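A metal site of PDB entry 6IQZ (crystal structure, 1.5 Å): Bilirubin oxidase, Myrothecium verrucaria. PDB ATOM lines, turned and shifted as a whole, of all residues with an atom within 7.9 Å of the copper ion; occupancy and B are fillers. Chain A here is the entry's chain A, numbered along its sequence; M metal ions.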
ATOM      1  N   ASN A 201     -22.599  24.456 -37.471  1.00  0.00           N
ATOM      2  CA  ASN A 201     -21.330  23.780 -37.174  1.00  0.00           C
ATOM      3  C   ASN A 201     -20.602  24.457 -36.013  1.00  0.00           C
ATOM      4  O   ASN A 201     -20.434  23.864 -34.959  1.00  0.00           O
ATOM      5  CB  ASN A 201     -20.448  23.758 -38.434  1.00  0.00           C
ATOM      6  CG  ASN A 201     -19.080  23.142 -38.174  1.00  0.00           C
ATOM      7  OD1 ASN A 201     -18.970  22.057 -37.611  1.00  0.00           O
ATOM      8  ND2 ASN A 201     -18.028  23.857 -38.577  1.00  0.00           N
ATOM      9  N   SER A 202     -20.155  25.697 -36.218  1.00  0.00           N
ATOM     10  CA  SER A 202     -19.530  26.511 -35.181  1.00  0.00           C
ATOM     11  C   SER A 202     -19.438  27.939 -35.671  1.00  0.00           C
ATOM     12  O   SER A 202     -19.233  28.188 -36.856  1.00  0.00           O
ATOM     13  CB  SER A 202     -18.125  26.016 -34.816  1.00  0.00           C
ATOM     14  OG  SER A 202     -18.138  24.971 -33.858  1.00  0.00           O
ATOM     15  N   MET A 277     -14.799  27.456 -24.026  1.00  0.00           N
ATOM     16  CA  MET A 277     -16.033  28.139 -23.701  1.00  0.00           C
ATOM     17  C   MET A 277     -16.543  27.774 -22.313  1.00  0.00           C
ATOM     18  O   MET A 277     -16.631  26.578 -21.962  1.00  0.00           O
ATOM     19  CB  MET A 277     -17.118  27.836 -24.744  1.00  0.00           C
ATOM     20  CG  MET A 277     -16.877  28.449 -26.136  1.00  0.00           C
ATOM     21  SD  MET A 277     -15.573  27.634 -27.094  1.00  0.00           S
ATOM     22  CE  MET A 277     -16.413  26.140 -27.630  1.00  0.00           C
ATOM     23  N   PHE A 358     -19.692  12.356 -27.227  1.00  0.00           N
ATOM     24  CA  PHE A 358     -20.061  13.646 -27.787  1.00  0.00           C
ATOM     25  C   PHE A 358     -19.716  13.644 -29.262  1.00  0.00           C
ATOM     26  O   PHE A 358     -18.545  13.600 -29.643  1.00  0.00           O
ATOM     27  CB  PHE A 358     -19.355  14.767 -27.034  1.00  0.00           C
ATOM     28  CG  PHE A 358     -19.733  14.806 -25.594  1.00  0.00           C
ATOM     29  CD1 PHE A 358     -19.057  14.041 -24.662  1.00  0.00           C
ATOM     30  CD2 PHE A 358     -20.819  15.560 -25.171  1.00  0.00           C
ATOM     31  CE1 PHE A 358     -19.431  14.026 -23.333  1.00  0.00           C
ATOM     32  CE2 PHE A 358     -21.211  15.555 -23.848  1.00  0.00           C
ATOM     33  CZ  PHE A 358     -20.513  14.791 -22.919  1.00  0.00           C
ATOM     34  N   GLY A 359     -20.741  13.688 -30.109  1.00  0.00           N
ATOM     35  CA  GLY A 359     -20.536  13.584 -31.546  1.00  0.00           C
ATOM     36  C   GLY A 359     -21.742  14.016 -32.340  1.00  0.00           C
ATOM     37  O   GLY A 359     -22.568  14.790 -31.875  1.00  0.00           O
ATOM     38  N   TRP A 365     -25.880  17.536 -33.368  1.00  0.00           N
ATOM     39  CA  TRP A 365     -24.901  17.329 -32.314  1.00  0.00           C
ATOM     40  C   TRP A 365     -25.597  16.627 -31.158  1.00  0.00           C
ATOM     41  O   TRP A 365     -26.634  17.088 -30.686  1.00  0.00           O
ATOM     42  CB  TRP A 365     -24.297  18.668 -31.886  1.00  0.00           C
ATOM     43  CG  TRP A 365     -23.515  19.373 -32.958  1.00  0.00           C
ATOM     44  CD1 TRP A 365     -23.898  20.485 -33.672  1.00  0.00           C
ATOM     45  CD2 TRP A 365     -22.215  19.012 -33.437  1.00  0.00           C
ATOM     46  NE1 TRP A 365     -22.891  20.836 -34.552  1.00  0.00           N
ATOM     47  CE2 TRP A 365     -21.846  19.962 -34.422  1.00  0.00           C
ATOM     48  CE3 TRP A 365     -21.305  17.999 -33.115  1.00  0.00           C
ATOM     49  CZ2 TRP A 365     -20.638  19.900 -35.111  1.00  0.00           C
ATOM     50  CZ3 TRP A 365     -20.096  17.943 -33.796  1.00  0.00           C
ATOM     51  CH2 TRP A 365     -19.771  18.893 -34.774  1.00  0.00           C
ATOM     52  N   THR A 366     -25.023  15.510 -30.688  1.00  0.00           N
ATOM     53  CA  THR A 366     -25.714  14.667 -29.717  1.00  0.00           C
ATOM     54  C   THR A 366     -24.817  14.175 -28.584  1.00  0.00           C
ATOM     55  O   THR A 366     -23.591  14.212 -28.681  1.00  0.00           O
ATOM     56  CB  THR A 366     -26.319  13.420 -30.391  1.00  0.00           C
ATOM     57  OG1 THR A 366     -25.297  12.712 -31.104  1.00  0.00           O
ATOM     58  CG2 THR A 366     -27.437  13.801 -31.364  1.00  0.00           C
ATOM     59  N   ASN A 395     -14.620  12.236 -26.730  1.00  0.00           N
ATOM     60  CA  ASN A 395     -14.670  12.813 -28.070  1.00  0.00           C
ATOM     61  C   ASN A 395     -13.858  11.950 -29.010  1.00  0.00           C
ATOM     62  O   ASN A 395     -12.630  11.986 -28.980  1.00  0.00           O
ATOM     63  CB  ASN A 395     -14.133  14.247 -28.070  1.00  0.00           C
ATOM     64  CG  ASN A 395     -14.136  14.857 -29.456  1.00  0.00           C
ATOM     65  OD1 ASN A 395     -14.823  14.366 -30.348  1.00  0.00           O
ATOM     66  ND2 ASN A 395     -13.362  15.928 -29.639  1.00  0.00           N
ATOM     67  N   TRP A 400     -14.197  18.022 -34.388  1.00  0.00           N
ATOM     68  CA  TRP A 400     -14.853  18.943 -33.468  1.00  0.00           C
ATOM     69  C   TRP A 400     -14.195  18.839 -32.108  1.00  0.00           C
ATOM     70  O   TRP A 400     -13.503  17.855 -31.822  1.00  0.00           O
ATOM     71  CB  TRP A 400     -16.371  18.651 -33.357  1.00  0.00           C
ATOM     72  CG  TRP A 400     -16.726  17.246 -32.928  1.00  0.00           C
ATOM     73  CD1 TRP A 400     -17.070  16.823 -31.664  1.00  0.00           C
ATOM     74  CD2 TRP A 400     -16.761  16.072 -33.755  1.00  0.00           C
ATOM     75  NE1 TRP A 400     -17.312  15.475 -31.664  1.00  0.00           N
ATOM     76  CE2 TRP A 400     -17.140  14.985 -32.930  1.00  0.00           C
ATOM     77  CE3 TRP A 400     -16.522  15.836 -35.110  1.00  0.00           C
ATOM     78  CZ2 TRP A 400     -17.258  13.694 -33.414  1.00  0.00           C
ATOM     79  CZ3 TRP A 400     -16.648  14.541 -35.589  1.00  0.00           C
ATOM     80  CH2 TRP A 400     -17.020  13.483 -34.750  1.00  0.00           C
ATOM     81  N   THR A 401     -14.395  19.856 -31.288  1.00  0.00           N
ATOM     82  CA  THR A 401     -14.000  19.791 -29.875  1.00  0.00           C
ATOM     83  C   THR A 401     -15.159  20.315 -29.037  1.00  0.00           C
ATOM     84  O   THR A 401     -16.027  21.057 -29.528  1.00  0.00           O
ATOM     85  CB  THR A 401     -12.732  20.598 -29.550  1.00  0.00           C
ATOM     86  OG1 THR A 401     -13.024  22.006 -29.554  1.00  0.00           O
ATOM     87  CG2 THR A 401     -11.593  20.273 -30.509  1.00  0.00           C
ATOM     88  N   HIS A 402     -15.155  19.958 -27.755  1.00  0.00           N
ATOM     89  CA  HIS A 402     -16.365  20.057 -26.941  1.00  0.00           C
ATOM     90  C   HIS A 402     -16.017  20.332 -25.486  1.00  0.00           C
ATOM     91  O   HIS A 402     -15.551  19.442 -24.777  1.00  0.00           O
ATOM     92  CB  HIS A 402     -17.162  18.756 -27.048  1.00  0.00           C
ATOM     93  CG  HIS A 402     -17.414  18.354 -28.461  1.00  0.00           C
ATOM     94  ND1 HIS A 402     -18.406  18.932 -29.224  1.00  0.00           N
ATOM     95  CD2 HIS A 402     -16.781  17.475 -29.269  1.00  0.00           C
ATOM     96  CE1 HIS A 402     -18.389  18.416 -30.444  1.00  0.00           C
ATOM     97  NE2 HIS A 402     -17.405  17.533 -30.499  1.00  0.00           N
ATOM     98  N   PRO A 403     -16.245  21.561 -25.037  1.00  0.00           N
ATOM     99  CA  PRO A 403     -16.070  21.847 -23.612  1.00  0.00           C
ATOM    100  C   PRO A 403     -17.334  21.479 -22.841  1.00  0.00           C
ATOM    101  O   PRO A 403     -18.376  22.114 -23.044  1.00  0.00           O
ATOM    102  CB  PRO A 403     -15.783  23.358 -23.603  1.00  0.00           C
ATOM    103  CG  PRO A 403     -16.480  23.899 -24.819  1.00  0.00           C
ATOM    104  CD  PRO A 403     -16.517  22.771 -25.832  1.00  0.00           C
ATOM    105  N   ILE A 404     -17.231  20.463 -21.987  1.00  0.00           N
ATOM    106  CA  ILE A 404     -18.420  19.892 -21.378  1.00  0.00           C
ATOM    107  C   ILE A 404     -18.672  20.457 -19.992  1.00  0.00           C
ATOM    108  O   ILE A 404     -17.790  20.478 -19.144  1.00  0.00           O
ATOM    109  CB  ILE A 404     -18.301  18.353 -21.258  1.00  0.00           C
ATOM    110  CG1 ILE A 404     -17.974  17.743 -22.624  1.00  0.00           C
ATOM    111  CG2 ILE A 404     -19.583  17.759 -20.667  1.00  0.00           C
ATOM    112  CD1 ILE A 404     -18.886  18.188 -23.730  1.00  0.00           C
ATOM    113  N   LEU A 438     -12.791  18.823 -24.080  1.00  0.00           N
ATOM    114  CA  LEU A 438     -12.413  17.662 -24.872  1.00  0.00           C
ATOM    115  C   LEU A 438     -11.893  18.152 -26.206  1.00  0.00           C
ATOM    116  O   LEU A 438     -12.661  18.481 -27.110  1.00  0.00           O
ATOM    117  CB  LEU A 438     -13.602  16.706 -25.086  1.00  0.00           C
ATOM    118  CG  LEU A 438     -14.488  16.329 -23.903  1.00  0.00           C
ATOM    119  CD1 LEU A 438     -15.543  15.319 -24.352  1.00  0.00           C
ATOM    120  CD2 LEU A 438     -13.664  15.761 -22.764  1.00  0.00           C
ATOM    121  N   HIS A 460     -24.034  19.456 -20.818  1.00  0.00           N
ATOM    122  CA  HIS A 460     -24.000  19.773 -22.228  1.00  0.00           C
ATOM    123  C   HIS A 460     -22.644  20.281 -22.665  1.00  0.00           C
ATOM    124  O   HIS A 460     -21.811  20.649 -21.845  1.00  0.00           O
ATOM    125  CB  HIS A 460     -25.051  20.831 -22.560  1.00  0.00           C
ATOM    126  CG  HIS A 460     -24.896  22.090 -21.756  1.00  0.00           C
ATOM    127  ND1 HIS A 460     -24.168  23.169 -22.202  1.00  0.00           N
ATOM    128  CD2 HIS A 460     -25.368  22.421 -20.534  1.00  0.00           C
ATOM    129  CE1 HIS A 460     -24.204  24.126 -21.288  1.00  0.00           C
ATOM    130  NE2 HIS A 460     -24.923  23.695 -20.270  1.00  0.00           N
ATOM    131  N   CYS A 461     -22.452  20.306 -23.970  1.00  0.00           N
ATOM    132  CA  CYS A 461     -21.338  21.037 -24.548  1.00  0.00           C
ATOM    133  C   CYS A 461     -21.603  22.507 -24.440  1.00  0.00           C
ATOM    134  O   CYS A 461     -22.747  22.939 -24.611  1.00  0.00           O
ATOM    135  CB  CYS A 461     -21.158  20.650 -26.008  1.00  0.00           C
ATOM    136  SG  CYS A 461     -19.822  21.521 -26.768  1.00  0.00           S
ATOM    137  N   HIS A 462     -20.554  23.306 -24.185  1.00  0.00           N
ATOM    138  CA  HIS A 462     -20.740  24.750 -24.058  1.00  0.00           C
ATOM    139  C   HIS A 462     -20.267  25.534 -25.289  1.00  0.00           C
ATOM    140  O   HIS A 462     -20.174  26.752 -25.240  1.00  0.00           O
ATOM    141  CB  HIS A 462     -20.027  25.279 -22.807  1.00  0.00           C
ATOM    142  CG  HIS A 462     -20.820  26.315 -22.052  1.00  0.00           C
ATOM    143  ND1 HIS A 462     -21.051  27.581 -22.542  1.00  0.00           N
ATOM    144  CD2 HIS A 462     -21.422  26.256 -20.842  1.00  0.00           C
ATOM    145  CE1 HIS A 462     -21.756  28.268 -21.652  1.00  0.00           C
ATOM    146  NE2 HIS A 462     -21.993  27.487 -20.615  1.00  0.00           N
ATOM    147  N   ASN A 463     -20.007  24.830 -26.382  1.00  0.00           N
ATOM    148  CA  ASN A 463     -20.022  25.458 -27.704  1.00  0.00           C
ATOM    149  C   ASN A 463     -21.481  25.714 -27.992  1.00  0.00           C
ATOM    150  O   ASN A 463     -22.246  24.763 -28.129  1.00  0.00           O
ATOM    151  CB  ASN A 463     -19.392  24.526 -28.763  1.00  0.00           C
ATOM    152  CG  ASN A 463     -19.381  25.132 -30.148  1.00  0.00           C
ATOM    153  OD1 ASN A 463     -20.322  25.815 -30.544  1.00  0.00           O
ATOM    154  ND2 ASN A 463     -18.307  24.901 -30.889  1.00  0.00           N
ATOM    155  N   LEU A 464     -21.891  26.984 -28.037  1.00  0.00           N
ATOM    156  CA  LEU A 464     -23.313  27.262 -28.006  1.00  0.00           C
ATOM    157  C   LEU A 464     -24.021  26.850 -29.295  1.00  0.00           C
ATOM    158  O   LEU A 464     -25.225  26.593 -29.264  1.00  0.00           O
ATOM    159  CB  LEU A 464     -23.545  28.744 -27.722  1.00  0.00           C
ATOM    160  CG  LEU A 464     -22.934  29.232 -26.423  1.00  0.00           C
ATOM    161  CD1 LEU A 464     -23.326  30.684 -26.203  1.00  0.00           C
ATOM    162  CD2 LEU A 464     -23.402  28.371 -25.274  1.00  0.00           C
ATOM    163  N   ILE A 465     -23.301  26.773 -30.397  1.00  0.00           N
ATOM    164  CA  ILE A 465     -23.872  26.228 -31.635  1.00  0.00           C
ATOM    165  C   ILE A 465     -24.183  24.733 -31.462  1.00  0.00           C
ATOM    166  O   ILE A 465     -25.261  24.261 -31.821  1.00  0.00           O
ATOM    167  CB  ILE A 465     -22.928  26.438 -32.840  1.00  0.00           C
ATOM    168  CG1 ILE A 465     -22.702  27.929 -33.096  1.00  0.00           C
ATOM    169  CG2 ILE A 465     -23.481  25.767 -34.099  1.00  0.00           C
ATOM    170  CD1 ILE A 465     -23.984  28.717 -33.400  1.00  0.00           C
ATOM    171  N   HIS A 466     -23.258  23.998 -30.847  1.00  0.00           N
ATOM    172  CA  HIS A 466     -23.495  22.569 -30.610  1.00  0.00           C
ATOM    173  C   HIS A 466     -24.649  22.389 -29.645  1.00  0.00           C
ATOM    174  O   HIS A 466     -25.518  21.530 -29.847  1.00  0.00           O
ATOM    175  CB  HIS A 466     -22.253  21.889 -30.027  1.00  0.00           C
ATOM    176  CG  HIS A 466     -21.056  21.916 -30.934  1.00  0.00           C
ATOM    177  ND1 HIS A 466     -19.830  21.441 -30.555  1.00  0.00           N
ATOM    178  CD2 HIS A 466     -20.903  22.362 -32.209  1.00  0.00           C
ATOM    179  CE1 HIS A 466     -18.961  21.598 -31.542  1.00  0.00           C
ATOM    180  NE2 HIS A 466     -19.598  22.144 -32.557  1.00  0.00           N
ATOM    181  N   GLU A 467     -24.632  23.189 -28.583  1.00  0.00           N
ATOM    182  CA  GLU A 467     -25.655  23.119 -27.546  1.00  0.00           C
ATOM    183  C   GLU A 467     -27.065  23.324 -28.121  1.00  0.00           C
ATOM    184  O   GLU A 467     -28.001  22.624 -27.761  1.00  0.00           O
ATOM    185  CB  GLU A 467     -25.340  24.149 -26.455  1.00  0.00           C
ATOM    186  CG  GLU A 467     -26.320  24.175 -25.296  1.00  0.00           C
ATOM    187  CD  GLU A 467     -25.967  25.250 -24.284  1.00  0.00           C
ATOM    188  OE1 GLU A 467     -24.768  25.592 -24.177  1.00  0.00           O
ATOM    189  OE2 GLU A 467     -26.885  25.771 -23.612  1.00  0.00           O
ATOM    190  N   MET A 471     -26.797  19.394 -28.468  1.00  0.00           N
ATOM    191  CA  MET A 471     -25.889  18.578 -27.637  1.00  0.00           C
ATOM    192  C   MET A 471     -26.058  18.873 -26.160  1.00  0.00           C
ATOM    193  O   MET A 471     -25.176  19.448 -25.505  1.00  0.00           O
ATOM    194  CB  MET A 471     -24.436  18.832 -28.062  1.00  0.00           C
ATOM    195  CG  MET A 471     -23.413  17.833 -27.517  1.00  0.00           C
ATOM    196  SD  MET A 471     -21.771  18.172 -28.192  1.00  0.00           S
ATOM    197  CE  MET A 471     -21.629  16.866 -29.404  1.00  0.00           C
HETATM  198 CU    CU M   1     -19.498  20.605 -28.699  1.00  0.00          CU
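The copper ion is bound by ND1 of His 466, ND1 of His 402 and SG of Cys 461.
The backbone carbonyl oxygen (O) of Trp 365 lies within hydrogen-bond range of the backbone NH (N) of Met 471, at 3.2 Å. N of His 466 is in hydrogen-bond range of OD1 of Asn 463 (3.5 Å). SG of Cys 461 lies close to N of Asn 463. N of Met 471 lies within hydrogen-bond range of O of His 466 (2.8 Å). The side-chain amide oxygen (OD1) of Asn 463 is in hydrogen-bond range of the backbone NH (N) of Ile 465 (3.1 Å). N of Leu 438 is in hydrogen-bond range of O of His 402, 2.9 Å away. ND2 of Asn 463 sits at hydrogen-bond distance from OG of Ser 202, at 3.0 Å. The side-chain hydroxyl of Ser 202 is in hydrogen-bond range of a ring nitrogen (NE2) of His 466 (3.4 Å).
Thr 401 touches the copper ion (O to CU, 3.6 Å). CB of Asn 463 touches the copper ion (3.9 Å). Met 471 touches the copper ion (SD to CU, 3.4 Å). Of the 23 residues printed, 6 come within 4 Å of the copper ion. The nearest printed residue that does not touch the copper ion is Pro 403 (4.7 Å).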
